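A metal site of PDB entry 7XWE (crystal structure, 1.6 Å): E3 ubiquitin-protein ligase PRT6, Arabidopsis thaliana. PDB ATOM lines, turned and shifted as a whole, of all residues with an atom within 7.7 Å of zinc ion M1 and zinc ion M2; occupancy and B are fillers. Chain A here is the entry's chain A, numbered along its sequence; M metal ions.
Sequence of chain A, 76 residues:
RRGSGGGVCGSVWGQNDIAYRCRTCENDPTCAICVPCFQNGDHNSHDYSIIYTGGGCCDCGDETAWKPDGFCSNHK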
ATOM      1  N   SER A   4      10.409   8.397   6.999  1.00  0.00           N
ATOM      2  CA  SER A   4       9.803   8.127   8.297  1.00  0.00           C
ATOM      3  C   SER A   4      10.412   6.862   8.879  1.00  0.00           C
ATOM      4  O   SER A   4      11.083   6.080   8.193  1.00  0.00           O
ATOM      5  CB  SER A   4       8.277   7.994   8.200  1.00  0.00           C
ATOM      6  OG  SER A   4       7.680   8.237   9.473  1.00  0.00           O
ATOM      7  N   GLY A   7      12.711   6.395  14.349  1.00  0.00           N
ATOM      8  CA  GLY A   7      12.421   7.256  15.481  1.00  0.00           C
ATOM      9  C   GLY A   7      12.040   8.657  15.099  1.00  0.00           C
ATOM     10  O   GLY A   7      12.308   9.595  15.859  1.00  0.00           O
ATOM     11  N   VAL A   8      11.446   8.839  13.929  1.00  0.00           N
ATOM     12  CA  VAL A   8      11.076  10.147  13.409  1.00  0.00           C
ATOM     13  C   VAL A   8       9.829   9.952  12.565  1.00  0.00           C
ATOM     14  O   VAL A   8       9.732   8.983  11.806  1.00  0.00           O
ATOM     15  CB  VAL A   8      12.212  10.763  12.567  1.00  0.00           C
ATOM     16  CG1 VAL A   8      12.511   9.874  11.369  1.00  0.00           C
ATOM     17  CG2 VAL A   8      11.846  12.158  12.117  1.00  0.00           C
ATOM     18  N   CYS A   9       8.878  10.880  12.677  1.00  0.00           N
ATOM     19  CA  CYS A   9       7.656  10.777  11.892  1.00  0.00           C
ATOM     20  C   CYS A   9       7.845  11.292  10.474  1.00  0.00           C
ATOM     21  O   CYS A   9       7.598  10.579   9.498  1.00  0.00           O
ATOM     22  CB  CYS A   9       6.516  11.522  12.571  1.00  0.00           C
ATOM     23  SG  CYS A   9       4.974  11.512  11.601  1.00  0.00           S
ATOM     24  N   GLY A  10       8.187  12.568  10.336  1.00  0.00           N
ATOM     25  CA  GLY A  10       8.413  13.183   9.042  1.00  0.00           C
ATOM     26  C   GLY A  10       7.205  13.416   8.147  1.00  0.00           C
ATOM     27  O   GLY A  10       7.395  13.949   7.047  1.00  0.00           O
ATOM     28  N   SER A  11       5.998  13.020   8.550  1.00  0.00           N
ATOM     29  CA  SER A  11       4.810  13.279   7.735  1.00  0.00           C
ATOM     30  C   SER A  11       4.825  14.703   7.187  1.00  0.00           C
ATOM     31  O   SER A  11       5.085  15.656   7.933  1.00  0.00           O
ATOM     32  CB  SER A  11       3.529  13.061   8.538  1.00  0.00           C
ATOM     33  OG  SER A  11       3.118  11.715   8.526  1.00  0.00           O
ATOM     34  N   VAL A  12       4.533  14.855   5.897  1.00  0.00           N
ATOM     35  CA  VAL A  12       4.611  16.150   5.215  1.00  0.00           C
ATOM     36  C   VAL A  12       3.197  16.650   4.948  1.00  0.00           C
ATOM     37  O   VAL A  12       2.350  15.891   4.450  1.00  0.00           O
ATOM     38  CB  VAL A  12       5.413  16.073   3.915  1.00  0.00           C
ATOM     39  CG1 VAL A  12       5.235  17.352   3.090  1.00  0.00           C
ATOM     40  CG2 VAL A  12       6.884  15.800   4.194  1.00  0.00           C
ATOM     41  N   TRP A  13       2.950  17.912   5.258  1.00  0.00           N
ATOM     42  CA  TRP A  13       1.630  18.514   5.109  1.00  0.00           C
ATOM     43  C   TRP A  13       1.515  19.336   3.821  1.00  0.00           C
ATOM     44  O   TRP A  13       2.489  19.929   3.359  1.00  0.00           O
ATOM     45  CB  TRP A  13       1.306  19.445   6.283  1.00  0.00           C
ATOM     46  CG  TRP A  13       1.213  18.767   7.609  1.00  0.00           C
ATOM     47  CD1 TRP A  13       0.413  17.733   7.957  1.00  0.00           C
ATOM     48  CD2 TRP A  13       1.982  19.091   8.783  1.00  0.00           C
ATOM     49  NE1 TRP A  13       0.629  17.381   9.278  1.00  0.00           N
ATOM     50  CE2 TRP A  13       1.589  18.203   9.801  1.00  0.00           C
ATOM     51  CE3 TRP A  13       2.965  20.051   9.065  1.00  0.00           C
ATOM     52  CZ2 TRP A  13       2.136  18.251  11.082  1.00  0.00           C
ATOM     53  CZ3 TRP A  13       3.511  20.094  10.334  1.00  0.00           C
ATOM     54  CH2 TRP A  13       3.088  19.193  11.328  1.00  0.00           C
ATOM     55  N   ALA A  32       5.087  21.650  15.331  1.00  0.00           N
ATOM     56  CA  ALA A  32       3.746  21.058  15.303  1.00  0.00           C
ATOM     57  C   ALA A  32       3.877  19.565  15.111  1.00  0.00           C
ATOM     58  O   ALA A  32       4.898  19.080  14.622  1.00  0.00           O
ATOM     59  CB  ALA A  32       2.888  21.659  14.188  1.00  0.00           C
ATOM     60  N   ILE A  33       2.828  18.840  15.483  1.00  0.00           N
ATOM     61  CA  ILE A  33       2.824  17.390  15.236  1.00  0.00           C
ATOM     62  C   ILE A  33       1.516  16.997  14.577  1.00  0.00           C
ATOM     63  O   ILE A  33       0.469  17.629  14.780  1.00  0.00           O
ATOM     64  CB  ILE A  33       3.058  16.536  16.505  1.00  0.00           C
ATOM     65  CG1 ILE A  33       1.993  16.788  17.572  1.00  0.00           C
ATOM     66  CG2 ILE A  33       4.495  16.797  17.064  1.00  0.00           C
ATOM     67  CD1 ILE A  33       2.066  15.764  18.728  1.00  0.00           C
ATOM     68  N   CYS A  34       1.577  15.925  13.804  1.00  0.00           N
ATOM     69  CA  CYS A  34       0.424  15.486  13.036  1.00  0.00           C
ATOM     70  C   CYS A  34      -0.648  14.887  13.958  1.00  0.00           C
ATOM     71  O   CYS A  34      -0.384  14.509  15.109  1.00  0.00           O
ATOM     72  CB  CYS A  34       0.866  14.498  11.963  1.00  0.00           C
ATOM     73  SG  CYS A  34       1.359  12.864  12.546  1.00  0.00           S
ATOM     74  N   VAL A  35      -1.881  14.854  13.461  1.00  0.00           N
ATOM     75  CA  VAL A  35      -2.995  14.399  14.292  1.00  0.00           C
ATOM     76  C   VAL A  35      -2.785  12.982  14.819  1.00  0.00           C
ATOM     77  O   VAL A  35      -2.997  12.751  16.013  1.00  0.00           O
ATOM     78  CB  VAL A  35      -4.325  14.543  13.516  1.00  0.00           C
ATOM     79  CG1 VAL A  35      -5.449  13.955  14.344  1.00  0.00           C
ATOM     80  CG2 VAL A  35      -4.590  16.031  13.264  1.00  0.00           C
ATOM     81  N   PRO A  36      -2.347  12.007  14.003  1.00  0.00           N
ATOM     82  CA  PRO A  36      -2.077  10.657  14.573  1.00  0.00           C
ATOM     83  C   PRO A  36      -1.042  10.663  15.671  1.00  0.00           C
ATOM     84  O   PRO A  36      -1.215   9.981  16.674  1.00  0.00           O
ATOM     85  CB  PRO A  36      -1.577   9.862  13.356  1.00  0.00           C
ATOM     86  CG  PRO A  36      -2.155  10.571  12.163  1.00  0.00           C
ATOM     87  CD  PRO A  36      -2.232  12.024  12.531  1.00  0.00           C
ATOM     88  N   CYS A  37       0.062  11.393  15.502  1.00  0.00           N
ATOM     89  CA  CYS A  37       1.051  11.413  16.567  1.00  0.00           C
ATOM     90  C   CYS A  37       0.501  12.076  17.815  1.00  0.00           C
ATOM     91  O   CYS A  37       0.780  11.650  18.955  1.00  0.00           O
ATOM     92  CB  CYS A  37       2.290  12.192  16.110  1.00  0.00           C
ATOM     93  SG  CYS A  37       3.313  11.339  14.845  1.00  0.00           S
ATOM     94  N   PHE A  38      -0.300  13.160  17.683  1.00  0.00           N
ATOM     95  CA  PHE A  38      -0.934  13.760  18.850  1.00  0.00           C
ATOM     96  C   PHE A  38      -1.814  12.742  19.552  1.00  0.00           C
ATOM     97  O   PHE A  38      -1.756  12.600  20.779  1.00  0.00           O
ATOM     98  CB  PHE A  38      -1.772  14.978  18.453  1.00  0.00           C
ATOM     99  CG  PHE A  38      -2.428  15.646  19.630  1.00  0.00           C
ATOM    100  CD1 PHE A  38      -1.710  16.558  20.403  1.00  0.00           C
ATOM    101  CD2 PHE A  38      -3.707  15.331  19.980  1.00  0.00           C
ATOM    102  CE1 PHE A  38      -2.287  17.161  21.494  1.00  0.00           C
ATOM    103  CE2 PHE A  38      -4.299  15.937  21.055  1.00  0.00           C
ATOM    104  CZ  PHE A  38      -3.581  16.849  21.828  1.00  0.00           C
ATOM    105  N   ASN A  40      -1.643   9.551  19.567  1.00  0.00           N
ATOM    106  CA  ASN A  40      -0.884   8.448  20.144  1.00  0.00           C
ATOM    107  C   ASN A  40       0.133   8.904  21.201  1.00  0.00           C
ATOM    108  O   ASN A  40       1.001   8.118  21.608  1.00  0.00           O
ATOM    109  CB  ASN A  40      -0.204   7.667  19.030  1.00  0.00           C
ATOM    110  CG  ASN A  40      -1.180   6.852  18.197  1.00  0.00           C
ATOM    111  OD1 ASN A  40      -1.186   6.909  16.965  1.00  0.00           O
ATOM    112  ND2 ASN A  40      -1.970   6.035  18.866  1.00  0.00           N
ATOM    113  N   GLY A  41      -0.002  10.140  21.708  1.00  0.00           N
ATOM    114  CA  GLY A  41       0.857  10.627  22.764  1.00  0.00           C
ATOM    115  C   GLY A  41       0.055  11.093  23.980  1.00  0.00           C
ATOM    116  O   GLY A  41      -1.163  10.943  24.043  1.00  0.00           O
ATOM    117  N   CYS A  57       6.334  19.775   8.078  1.00  0.00           N
ATOM    118  CA  CYS A  57       6.398  18.373   8.409  1.00  0.00           C
ATOM    119  C   CYS A  57       6.298  18.196   9.911  1.00  0.00           C
ATOM    120  O   CYS A  57       6.635  19.084  10.695  1.00  0.00           O
ATOM    121  CB  CYS A  57       7.689  17.743   7.868  1.00  0.00           C
ATOM    122  SG  CYS A  57       9.162  18.225   8.730  1.00  0.00           S
ATOM    123  N   CYS A  58       5.799  17.019  10.305  1.00  0.00           N
ATOM    124  CA  CYS A  58       5.602  16.706  11.712  1.00  0.00           C
ATOM    125  C   CYS A  58       6.919  16.647  12.460  1.00  0.00           C
ATOM    126  O   CYS A  58       7.901  16.085  11.976  1.00  0.00           O
ATOM    127  CB  CYS A  58       4.891  15.353  11.836  1.00  0.00           C
ATOM    128  SG  CYS A  58       4.633  14.753  13.474  1.00  0.00           S
ATOM    129  N   ASP A  59       6.923  17.200  13.664  1.00  0.00           N
ATOM    130  CA  ASP A  59       8.136  17.248  14.475  1.00  0.00           C
ATOM    131  C   ASP A  59       8.267  16.095  15.449  1.00  0.00           C
ATOM    132  O   ASP A  59       9.247  16.048  16.181  1.00  0.00           O
ATOM    133  CB  ASP A  59       8.184  18.581  15.226  1.00  0.00           C
ATOM    134  CG  ASP A  59       8.362  19.750  14.288  1.00  0.00           C
ATOM    135  OD1 ASP A  59       9.217  19.665  13.390  1.00  0.00           O
ATOM    136  OD2 ASP A  59       7.618  20.728  14.431  1.00  0.00           O
ATOM    137  N   CYS A  60       7.305  15.175  15.481  1.00  0.00           N
ATOM    138  CA  CYS A  60       7.333  14.060  16.432  1.00  0.00           C
ATOM    139  C   CYS A  60       8.557  13.198  16.224  1.00  0.00           C
ATOM    140  O   CYS A  60       8.863  12.783  15.111  1.00  0.00           O
ATOM    141  CB  CYS A  60       6.057  13.233  16.255  1.00  0.00           C
ATOM    142  SG  CYS A  60       5.937  11.931  17.532  1.00  0.00           S
ATOM    143  N   GLY A  61       9.262  12.921  17.333  1.00  0.00           N
ATOM    144  CA  GLY A  61      10.493  12.165  17.317  1.00  0.00           C
ATOM    145  C   GLY A  61      11.763  12.976  17.130  1.00  0.00           C
ATOM    146  O   GLY A  61      12.856  12.405  17.214  1.00  0.00           O
ATOM    147  N   GLY A  70       6.654  14.364  24.931  1.00  0.00           N
ATOM    148  CA  GLY A  70       5.565  14.598  24.019  1.00  0.00           C
ATOM    149  C   GLY A  70       5.612  13.789  22.744  1.00  0.00           C
ATOM    150  O   GLY A  70       4.755  13.993  21.872  1.00  0.00           O
ATOM    151  N   PHE A  71       6.594  12.905  22.603  1.00  0.00           N
ATOM    152  CA  PHE A  71       6.645  11.983  21.470  1.00  0.00           C
ATOM    153  C   PHE A  71       5.487  10.997  21.586  1.00  0.00           C
ATOM    154  O   PHE A  71       5.100  10.600  22.681  1.00  0.00           O
ATOM    155  CB  PHE A  71       7.956  11.189  21.457  1.00  0.00           C
ATOM    156  CG  PHE A  71       9.205  12.001  21.124  1.00  0.00           C
ATOM    157  CD1 PHE A  71      10.445  11.406  21.253  1.00  0.00           C
ATOM    158  CD2 PHE A  71       9.149  13.317  20.691  1.00  0.00           C
ATOM    159  CE1 PHE A  71      11.604  12.114  20.974  1.00  0.00           C
ATOM    160  CE2 PHE A  71      10.314  14.012  20.408  1.00  0.00           C
ATOM    161  CZ  PHE A  71      11.533  13.414  20.533  1.00  0.00           C
ATOM    162  N   CYS A  72       4.944  10.591  20.437  1.00  0.00           N
ATOM    163  CA  CYS A  72       3.917   9.568  20.419  1.00  0.00           C
ATOM    164  C   CYS A  72       4.548   8.199  20.682  1.00  0.00           C
ATOM    165  O   CYS A  72       5.775   8.034  20.670  1.00  0.00           O
ATOM    166  CB  CYS A  72       3.170   9.575  19.075  1.00  0.00           C
ATOM    167  SG  CYS A  72       3.981   8.682  17.729  1.00  0.00           S
ATOM    168  N   SER A  73       3.693   7.207  20.907  1.00  0.00           N
ATOM    169  CA  SER A  73       4.157   5.875  21.283  1.00  0.00           C
ATOM    170  C   SER A  73       4.977   5.200  20.188  1.00  0.00           C
ATOM    171  O   SER A  73       5.717   4.251  20.467  1.00  0.00           O
ATOM    172  CB  SER A  73       2.954   5.010  21.635  1.00  0.00           C
ATOM    173  OG  SER A  73       2.167   4.817  20.467  1.00  0.00           O
ATOM    174  N   ASN A  74       4.872   5.683  18.948  1.00  0.00           N
ATOM    175  CA  ASN A  74       5.530   5.050  17.802  1.00  0.00           C
ATOM    176  C   ASN A  74       6.831   5.725  17.370  1.00  0.00           C
ATOM    177  O   ASN A  74       7.527   5.175  16.510  1.00  0.00           O
ATOM    178  CB  ASN A  74       4.572   5.014  16.618  1.00  0.00           C
ATOM    179  CG  ASN A  74       3.346   4.189  16.892  1.00  0.00           C
ATOM    180  OD1 ASN A  74       2.206   4.653  16.720  1.00  0.00           O
ATOM    181  ND2 ASN A  74       3.557   2.981  17.343  1.00  0.00           N
ATOM    182  N   HIS A  75       7.161   6.901  17.888  1.00  0.00           N
ATOM    183  CA  HIS A  75       8.388   7.593  17.509  1.00  0.00           C
ATOM    184  C   HIS A  75       9.265   7.840  18.739  1.00  0.00           C
ATOM    185  O   HIS A  75       9.978   8.858  18.824  1.00  0.00           O
ATOM    186  CB  HIS A  75       8.060   8.875  16.742  1.00  0.00           C
ATOM    187  CG  HIS A  75       7.294   8.611  15.479  1.00  0.00           C
ATOM    188  ND1 HIS A  75       6.027   9.105  15.249  1.00  0.00           N
ATOM    189  CD2 HIS A  75       7.600   7.848  14.396  1.00  0.00           C
ATOM    190  CE1 HIS A  75       5.596   8.679  14.085  1.00  0.00           C
ATOM    191  NE2 HIS A  75       6.528   7.924  13.543  1.00  0.00           N
ATOM    192  N   LYS A  76       9.185   6.889  19.658  1.00  0.00           N
ATOM    193  CA  LYS A  76       9.935   6.721  20.910  1.00  0.00           C
ATOM    194  C   LYS A  76       9.458   7.672  21.979  1.00  0.00           C
ATOM    195  O   LYS A  76       8.587   7.283  22.770  1.00  0.00           O
ATOM    196  CB  LYS A  76      11.429   6.834  20.662  1.00  0.00           C
ATOM    197  CG  LYS A  76      11.843   5.836  19.595  1.00  0.00           C
ATOM    198  CD  LYS A  76      13.255   5.341  19.775  1.00  0.00           C
ATOM    199  CE  LYS A  76      14.233   6.087  18.882  1.00  0.00           C
ATOM    200  NZ  LYS A  76      15.172   5.097  18.249  1.00  0.00           N
HETATM  201 ZN    ZN M   1       4.895  10.315  16.397  1.00  0.00          ZN
HETATM  202 ZN    ZN M   2       3.620  12.715  13.025  1.00  0.00          ZN
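The backbone carbonyl oxygen (O) of Cys 60 is in hydrogen-bond range of the backbone NH (N) of Cys 9, 3.1 Å away.
N of Cys 60 lies close to SG of Cys 58 (3.4 Å).
The backbone NH (N) of Asn 74 lies close to the side-chain sulfur (SG) of Cys 72 (3.4 Å).
The side-chain sulfur of Cys 9 lies close to the backbone NH of Ser 11, 3.6 Å away.
The backbone carbonyl oxygen of Ser 11 lies within hydrogen-bond range of the backbone NH of Cys 58, at 2.8 Å.
Four residues have an atom within 4 Å of zinc ion M1: Cys 37, Cys 60, Cys 72 and His 75.
Zinc ion M1 is bound by ND1 of His 75 (2.0 Å), SG of Cys 60 (2.2 Å), SG of Cys 72 (2.3 Å) and SG of Cys 37 (2.4 Å).
Zinc ion M2 is bound by SG of Cys 37 (2.3 Å), SG of Cys 9 (2.3 Å), SG of Cys 34 (2.3 Å) and SG of Cys 58 (2.3 Å).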
